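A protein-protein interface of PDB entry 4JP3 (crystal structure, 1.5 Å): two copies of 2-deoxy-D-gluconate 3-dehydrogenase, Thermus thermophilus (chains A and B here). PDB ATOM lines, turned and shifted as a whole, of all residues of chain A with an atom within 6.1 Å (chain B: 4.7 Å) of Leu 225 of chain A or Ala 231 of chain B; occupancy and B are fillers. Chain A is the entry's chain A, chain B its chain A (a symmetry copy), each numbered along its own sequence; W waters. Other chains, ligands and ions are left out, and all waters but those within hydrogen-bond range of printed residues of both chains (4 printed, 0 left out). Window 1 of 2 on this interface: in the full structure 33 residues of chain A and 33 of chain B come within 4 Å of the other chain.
O of Tyr 224 of chain A is in hydrogen-bond range of N of Asp 233 of chain B (3.3 Å).
The side-chain hydroxyl (OG1) of Thr 226 of chain A lies within hydrogen-bond range of the backbone NH (N) of Val 169 of chain A. The backbone carbonyl oxygen (O) of Leu 225 of chain A is in hydrogen-bond range of the side-chain amide nitrogen (ND2) of Asn 170 of chain A, at 3.0 Å. OD1 of Asn 170 of chain A lies within hydrogen-bond range of N of Gln 228 of chain A (3.1 Å). The backbone NH of Val 232 of chain B is in hydrogen-bond range of the backbone carbonyl oxygen of Cys 173 of chain B (3.0 Å). OD2 of Asp 233 of chain B sits at hydrogen-bond distance from N of Leu 237 of chain B (2.8 Å).
Among the printed residues, pairs that only touch across the chains: Glu 221 of chain A with Val 213 of chain B (3.4 Å), Tyr 224 of chain A with Val 232 of chain B (3.4 Å), Leu 225 of chain A with Ala 231 of chain B (3.6 Å), Thr 226 of chain A with Asp 233 of chain B (3.95 Å), Gln 228 of chain A with Ala 231 of chain B (3.5 Å) and Gln 228 of chain A with Leu 237 of chain B (3.8 Å).
Of the printed residues of chain B, Tyr 224 of chain A touches Val 232 (3.4 Å) and Asp 233 (3.3 Å). Of chain B, only Ala 231 (3.6 Å) comes within 4 Å of Leu 225 of chain A. Printed residues of chain B within 4 Å of Gln 228 of chain A: Ala 231 (3.5 Å) and Leu 237 (3.8 Å). Ala 229 of chain B touches none of the printed residues of chain A. Of the printed residues of chain A, Ala 231 of chain B touches Leu 225 and Gln 228. Of the printed residues of chain A, Val 232 of chain B touches Tyr 224 (3.4 Å). Of the printed residues of chain A, Asp 233 of chain B touches Tyr 224 and Thr 226. The nearest printed residue of chain A that does not touch Asp 233 of chain B is Gln 228 of chain A (4.3 Å).
Of the 15 printed residues of chain A, 5 touch a printed residue of chain B. Printed residues of chain A that touch a printed residue of chain B: Glu 221, Tyr 224, Leu 225, Thr 226 and Gln 228. Of the 8 printed residues of chain B, 5 touch a printed residue of chain A. Among the printed residues, no Asp or Glu carboxylate lies within 4 Å of a Lys or Arg side-chain nitrogen of the other chain.
Positions printed for both chains: 229 and 230. Of the 7 pairs that touch across the chains among the printed residues, none has its exchanged pair printed and touching as well.
Water W2 lies within hydrogen-bond range of OE1 of Gln 228 of chain A (2.7 Å), N of Ala 231 of chain B (3.0 Å) and O of Ala 229 of chain A (3.0 Å). Water W1 lies within hydrogen-bond range of the backbone carbonyl oxygen (O) of Ala 231 of chain B, the side-chain carboxylate (OD1) of Asp 233 of chain B and the backbone NH (N) of Thr 226 of chain A. Water W3 lies within hydrogen-bond range of the backbone carbonyl oxygen of Asp 233 of chain B and the side-chain hydroxyl of Tyr 224 of chain A. Water W4 lies within hydrogen-bond range of the side-chain carboxylate of Asp 233 of chain B, the backbone carbonyl oxygen of Thr 226 of chain A and the side-chain amide nitrogen of Gln 228 of chain A.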
ATOM      1  N   ARG A 168       2.596   3.677  -0.271  1.00  0.00           N
ATOM      2  CA  ARG A 168       3.614   4.705  -0.096  1.00  0.00           C
ATOM      3  C   ARG A 168       4.616   4.460  -1.219  1.00  0.00           C
ATOM      4  O   ARG A 168       4.962   3.312  -1.503  1.00  0.00           O
ATOM      5  CB  ARG A 168       4.296   4.571   1.268  1.00  0.00           C
ATOM      6  CG  ARG A 168       3.323   4.524   2.442  1.00  0.00           C
ATOM      7  CD  ARG A 168       2.482   5.799   2.553  1.00  0.00           C
ATOM      8  NE  ARG A 168       1.411   5.654   3.538  1.00  0.00           N
ATOM      9  CZ  ARG A 168       0.114   5.616   3.239  1.00  0.00           C
ATOM     10  NH1 ARG A 168      -0.289   5.716   1.980  1.00  0.00           N
ATOM     11  NH2 ARG A 168      -0.785   5.473   4.205  1.00  0.00           N
ATOM     12  N   VAL A 169       5.063   5.533  -1.867  1.00  0.00           N
ATOM     13  CA  VAL A 169       6.007   5.433  -2.981  1.00  0.00           C
ATOM     14  C   VAL A 169       7.182   6.361  -2.717  1.00  0.00           C
ATOM     15  O   VAL A 169       6.997   7.565  -2.569  1.00  0.00           O
ATOM     16  CB  VAL A 169       5.337   5.856  -4.308  1.00  0.00           C
ATOM     17  CG1 VAL A 169       6.291   5.628  -5.476  1.00  0.00           C
ATOM     18  CG2 VAL A 169       4.043   5.081  -4.509  1.00  0.00           C
ATOM     19  N   ASN A 170       8.385   5.800  -2.665  1.00  0.00           N
ATOM     20  CA  ASN A 170       9.577   6.592  -2.398  1.00  0.00           C
ATOM     21  C   ASN A 170      10.753   6.193  -3.272  1.00  0.00           C
ATOM     22  O   ASN A 170      10.752   5.126  -3.894  1.00  0.00           O
ATOM     23  CB  ASN A 170       9.959   6.471  -0.922  1.00  0.00           C
ATOM     24  CG  ASN A 170       8.917   7.078  -0.002  1.00  0.00           C
ATOM     25  OD1 ASN A 170       8.713   8.294   0.006  1.00  0.00           O
ATOM     26  ND2 ASN A 170       8.245   6.234   0.771  1.00  0.00           N
ATOM     27  N   VAL A 216      13.427  -0.041   5.838  1.00  0.00           N
ATOM     28  CA  VAL A 216      12.607   0.932   6.548  1.00  0.00           C
ATOM     29  C   VAL A 216      11.529   1.492   5.620  1.00  0.00           C
ATOM     30  O   VAL A 216      10.360   1.611   5.999  1.00  0.00           O
ATOM     31  CB  VAL A 216      13.484   2.092   7.073  1.00  0.00           C
ATOM     32  CG1 VAL A 216      12.616   3.235   7.572  1.00  0.00           C
ATOM     33  CG2 VAL A 216      14.389   1.583   8.188  1.00  0.00           C
ATOM     34  N   LEU A 217      11.926   1.822   4.397  1.00  0.00           N
ATOM     35  CA  LEU A 217      11.003   2.375   3.414  1.00  0.00           C
ATOM     36  C   LEU A 217      10.009   1.340   2.887  1.00  0.00           C
ATOM     37  O   LEU A 217       9.075   1.679   2.160  1.00  0.00           O
ATOM     38  CB  LEU A 217      11.795   3.003   2.263  1.00  0.00           C
ATOM     39  CG  LEU A 217      12.657   4.196   2.706  1.00  0.00           C
ATOM     40  CD1 LEU A 217      13.492   4.696   1.540  1.00  0.00           C
ATOM     41  CD2 LEU A 217      11.765   5.308   3.239  1.00  0.00           C
ATOM     42  N   GLU A 221       7.491   1.833   9.217  1.00  0.00           N
ATOM     43  CA  GLU A 221       8.176   3.072   9.568  1.00  0.00           C
ATOM     44  C   GLU A 221       7.827   4.177   8.580  1.00  0.00           C
ATOM     45  O   GLU A 221       7.859   5.361   8.921  1.00  0.00           O
ATOM     46  CB  GLU A 221       9.693   2.873   9.578  1.00  0.00           C
ATOM     47  CG  GLU A 221      10.166   1.896  10.629  1.00  0.00           C
ATOM     48  CD  GLU A 221      10.408   0.511  10.066  1.00  0.00           C
ATOM     49  OE1 GLU A 221       9.575   0.030   9.267  1.00  0.00           O
ATOM     50  OE2 GLU A 221      11.432  -0.096  10.434  1.00  0.00           O
ATOM     51  N   ALA A 222       7.480   3.787   7.357  1.00  0.00           N
ATOM     52  CA  ALA A 222       7.148   4.753   6.317  1.00  0.00           C
ATOM     53  C   ALA A 222       5.655   5.034   6.183  1.00  0.00           C
ATOM     54  O   ALA A 222       5.200   5.513   5.145  1.00  0.00           O
ATOM     55  CB  ALA A 222       7.706   4.275   4.980  1.00  0.00           C
ATOM     56  N   GLU A 223       4.889   4.759   7.233  1.00  0.00           N
ATOM     57  CA  GLU A 223       3.451   4.991   7.178  1.00  0.00           C
ATOM     58  C   GLU A 223       3.079   6.409   6.747  1.00  0.00           C
ATOM     59  O   GLU A 223       2.123   6.592   5.998  1.00  0.00           O
ATOM     60  CB  GLU A 223       2.810   4.667   8.531  1.00  0.00           C
ATOM     61  CG  GLU A 223       1.312   4.969   8.620  1.00  0.00           C
ATOM     62  CD  GLU A 223       0.530   4.501   7.404  1.00  0.00           C
ATOM     63  OE1 GLU A 223       0.730   3.354   6.959  1.00  0.00           O
ATOM     64  OE2 GLU A 223      -0.298   5.289   6.897  1.00  0.00           O
ATOM     65  N   TYR A 224       3.832   7.408   7.203  1.00  0.00           N
ATOM     66  CA  TYR A 224       3.537   8.795   6.839  1.00  0.00           C
ATOM     67  C   TYR A 224       4.646   9.381   5.961  1.00  0.00           C
ATOM     68  O   TYR A 224       4.781  10.603   5.839  1.00  0.00           O
ATOM     69  CB  TYR A 224       3.379   9.649   8.106  1.00  0.00           C
ATOM     70  CG  TYR A 224       2.524  10.885   7.914  1.00  0.00           C
ATOM     71  CD1 TYR A 224       1.143  10.779   7.749  1.00  0.00           C
ATOM     72  CD2 TYR A 224       3.095  12.159   7.879  1.00  0.00           C
ATOM     73  CE1 TYR A 224       0.348  11.906   7.554  1.00  0.00           C
ATOM     74  CE2 TYR A 224       2.309  13.294   7.682  1.00  0.00           C
ATOM     75  CZ  TYR A 224       0.937  13.158   7.518  1.00  0.00           C
ATOM     76  OH  TYR A 224       0.152  14.271   7.312  1.00  0.00           O
ATOM     77  N   LEU A 225       5.431   8.504   5.342  1.00  0.00           N
ATOM     78  CA  LEU A 225       6.535   8.930   4.487  1.00  0.00           C
ATOM     79  C   LEU A 225       6.267   8.496   3.050  1.00  0.00           C
ATOM     80  O   LEU A 225       6.302   7.303   2.733  1.00  0.00           O
ATOM     81  CB  LEU A 225       7.844   8.313   4.995  1.00  0.00           C
ATOM     82  CG  LEU A 225       9.172   8.981   4.617  1.00  0.00           C
ATOM     83  CD1 LEU A 225      10.304   8.298   5.380  1.00  0.00           C
ATOM     84  CD2 LEU A 225       9.412   8.904   3.117  1.00  0.00           C
ATOM     85  N   THR A 226       5.992   9.460   2.177  1.00  0.00           N
ATOM     86  CA  THR A 226       5.716   9.124   0.789  1.00  0.00           C
ATOM     87  C   THR A 226       5.975  10.282  -0.175  1.00  0.00           C
ATOM     88  O   THR A 226       5.842  11.453   0.193  1.00  0.00           O
ATOM     89  CB  THR A 226       4.255   8.620   0.637  1.00  0.00           C
ATOM     90  OG1 THR A 226       4.079   8.051  -0.664  1.00  0.00           O
ATOM     91  CG2 THR A 226       3.259   9.759   0.837  1.00  0.00           C
ATOM     92  N   GLY A 227       6.355   9.935  -1.404  1.00  0.00           N
ATOM     93  CA  GLY A 227       6.641  10.925  -2.432  1.00  0.00           C
ATOM     94  C   GLY A 227       7.988  11.597  -2.256  1.00  0.00           C
ATOM     95  O   GLY A 227       8.223  12.684  -2.788  1.00  0.00           O
ATOM     96  N   GLN A 228       8.885  10.936  -1.535  1.00  0.00           N
ATOM     97  CA  GLN A 228      10.196  11.498  -1.242  1.00  0.00           C
ATOM     98  C   GLN A 228      11.396  10.685  -1.680  1.00  0.00           C
ATOM     99  O   GLN A 228      11.317   9.474  -1.870  1.00  0.00           O
ATOM    100  CB  GLN A 228      10.332  11.714   0.266  1.00  0.00           C
ATOM    101  CG  GLN A 228       9.478  12.819   0.827  1.00  0.00           C
ATOM    102  CD  GLN A 228       9.915  14.168   0.317  1.00  0.00           C
ATOM    103  OE1 GLN A 228      11.101  14.495   0.346  1.00  0.00           O
ATOM    104  NE2 GLN A 228       8.963  14.965  -0.151  1.00  0.00           N
ATOM    105  N   ALA A 229      12.517  11.384  -1.823  1.00  0.00           N
ATOM    106  CA  ALA A 229      13.780  10.752  -2.151  1.00  0.00           C
ATOM    107  C   ALA A 229      14.525  10.731  -0.818  1.00  0.00           C
ATOM    108  O   ALA A 229      14.436  11.682  -0.038  1.00  0.00           O
ATOM    109  CB  ALA A 229      14.553  11.582  -3.169  1.00  0.00           C
ATOM    110  N   VAL A 230      15.225   9.637  -0.544  1.00  0.00           N
ATOM    111  CA  VAL A 230      16.007   9.504   0.677  1.00  0.00           C
ATOM    112  C   VAL A 230      17.394   9.096   0.207  1.00  0.00           C
ATOM    113  O   VAL A 230      17.582   7.991  -0.299  1.00  0.00           O
ATOM    114  CB  VAL A 230      15.427   8.416   1.615  1.00  0.00           C
ATOM    115  CG1 VAL A 230      16.313   8.258   2.844  1.00  0.00           C
ATOM    116  CG2 VAL A 230      14.010   8.796   2.036  1.00  0.00           C
ATOM    117  N   CYS B 173      12.282  16.216   8.690  1.00  0.00           N
ATOM    118  CA  CYS B 173      11.297  17.246   8.394  1.00  0.00           C
ATOM    119  C   CYS B 173       9.881  16.704   8.473  1.00  0.00           C
ATOM    120  O   CYS B 173       9.345  16.186   7.493  1.00  0.00           O
ATOM    121  CB  CYS B 173      11.543  17.832   7.001  1.00  0.00           C
ATOM    122  SG  CYS B 173      13.131  18.674   6.833  1.00  0.00           S
ATOM    123  N   VAL B 213      10.463   7.280  12.230  1.00  0.00           N
ATOM    124  CA  VAL B 213      11.554   7.632  11.329  1.00  0.00           C
ATOM    125  C   VAL B 213      12.704   8.267  12.105  1.00  0.00           C
ATOM    126  O   VAL B 213      13.871   8.040  11.794  1.00  0.00           O
ATOM    127  CB  VAL B 213      11.067   8.597  10.222  1.00  0.00           C
ATOM    128  CG1 VAL B 213      12.203   8.894   9.247  1.00  0.00           C
ATOM    129  CG2 VAL B 213       9.885   7.974   9.482  1.00  0.00           C
ATOM    130  N   ALA B 229      18.100  15.711   4.480  1.00  0.00           N
ATOM    131  CA  ALA B 229      16.806  16.033   5.049  1.00  0.00           C
ATOM    132  C   ALA B 229      15.938  14.838   4.659  1.00  0.00           C
ATOM    133  O   ALA B 229      16.070  14.304   3.555  1.00  0.00           O
ATOM    134  CB  ALA B 229      16.246  17.309   4.434  1.00  0.00           C
ATOM    135  N   VAL B 230      15.083  14.399   5.575  1.00  0.00           N
ATOM    136  CA  VAL B 230      14.176  13.289   5.318  1.00  0.00           C
ATOM    137  C   VAL B 230      12.801  13.817   5.695  1.00  0.00           C
ATOM    138  O   VAL B 230      12.526  14.062   6.868  1.00  0.00           O
ATOM    139  CB  VAL B 230      14.521  12.052   6.184  1.00  0.00           C
ATOM    140  CG1 VAL B 230      13.507  10.943   5.939  1.00  0.00           C
ATOM    141  CG2 VAL B 230      15.927  11.561   5.850  1.00  0.00           C
ATOM    142  N   ALA B 231      11.950  14.019   4.695  1.00  0.00           N
ATOM    143  CA  ALA B 231      10.613  14.548   4.929  1.00  0.00           C
ATOM    144  C   ALA B 231       9.580  13.447   5.128  1.00  0.00           C
ATOM    145  O   ALA B 231       9.450  12.544   4.301  1.00  0.00           O
ATOM    146  CB  ALA B 231      10.204  15.445   3.768  1.00  0.00           C
ATOM    147  N   VAL B 232       8.851  13.540   6.237  1.00  0.00           N
ATOM    148  CA  VAL B 232       7.805  12.585   6.598  1.00  0.00           C
ATOM    149  C   VAL B 232       6.563  13.465   6.686  1.00  0.00           C
ATOM    150  O   VAL B 232       6.187  13.930   7.765  1.00  0.00           O
ATOM    151  CB  VAL B 232       8.123  11.946   7.966  1.00  0.00           C
ATOM    152  CG1 VAL B 232       7.111  10.862   8.297  1.00  0.00           C
ATOM    153  CG2 VAL B 232       9.536  11.373   7.944  1.00  0.00           C
ATOM    154  N   ASP B 233       5.927  13.673   5.534  1.00  0.00           N
ATOM    155  CA  ASP B 233       4.794  14.586   5.429  1.00  0.00           C
ATOM    156  C   ASP B 233       3.516  14.096   4.757  1.00  0.00           C
ATOM    157  O   ASP B 233       2.708  14.915   4.313  1.00  0.00           O
ATOM    158  CB  ASP B 233       5.261  15.842   4.697  1.00  0.00           C
ATOM    159  CG  ASP B 233       5.595  15.570   3.235  1.00  0.00           C
ATOM    160  OD1 ASP B 233       5.482  14.400   2.803  1.00  0.00           O
ATOM    161  OD2 ASP B 233       5.967  16.522   2.516  1.00  0.00           O
ATOM    162  N   LEU B 237       4.679  17.703   0.281  1.00  0.00           N
ATOM    163  CA  LEU B 237       5.631  18.356  -0.612  1.00  0.00           C
ATOM    164  C   LEU B 237       5.584  17.832  -2.039  1.00  0.00           C
ATOM    165  O   LEU B 237       5.842  18.576  -2.984  1.00  0.00           O
ATOM    166  CB  LEU B 237       7.052  18.225  -0.053  1.00  0.00           C
ATOM    167  CG  LEU B 237       7.310  19.034   1.221  1.00  0.00           C
ATOM    168  CD1 LEU B 237       8.664  18.657   1.805  1.00  0.00           C
ATOM    169  CD2 LEU B 237       7.250  20.524   0.908  1.00  0.00           C
HETATM  170  O   HOH W   1       6.925  12.079   3.281  1.00  0.00           O
HETATM  171  O   HOH W   2      12.986  13.364   1.992  1.00  0.00           O
HETATM  172  O   HOH W   3       1.715  16.535   6.368  1.00  0.00           O
HETATM  173  O   HOH W   4       6.092  14.312   0.068  1.00  0.00           O
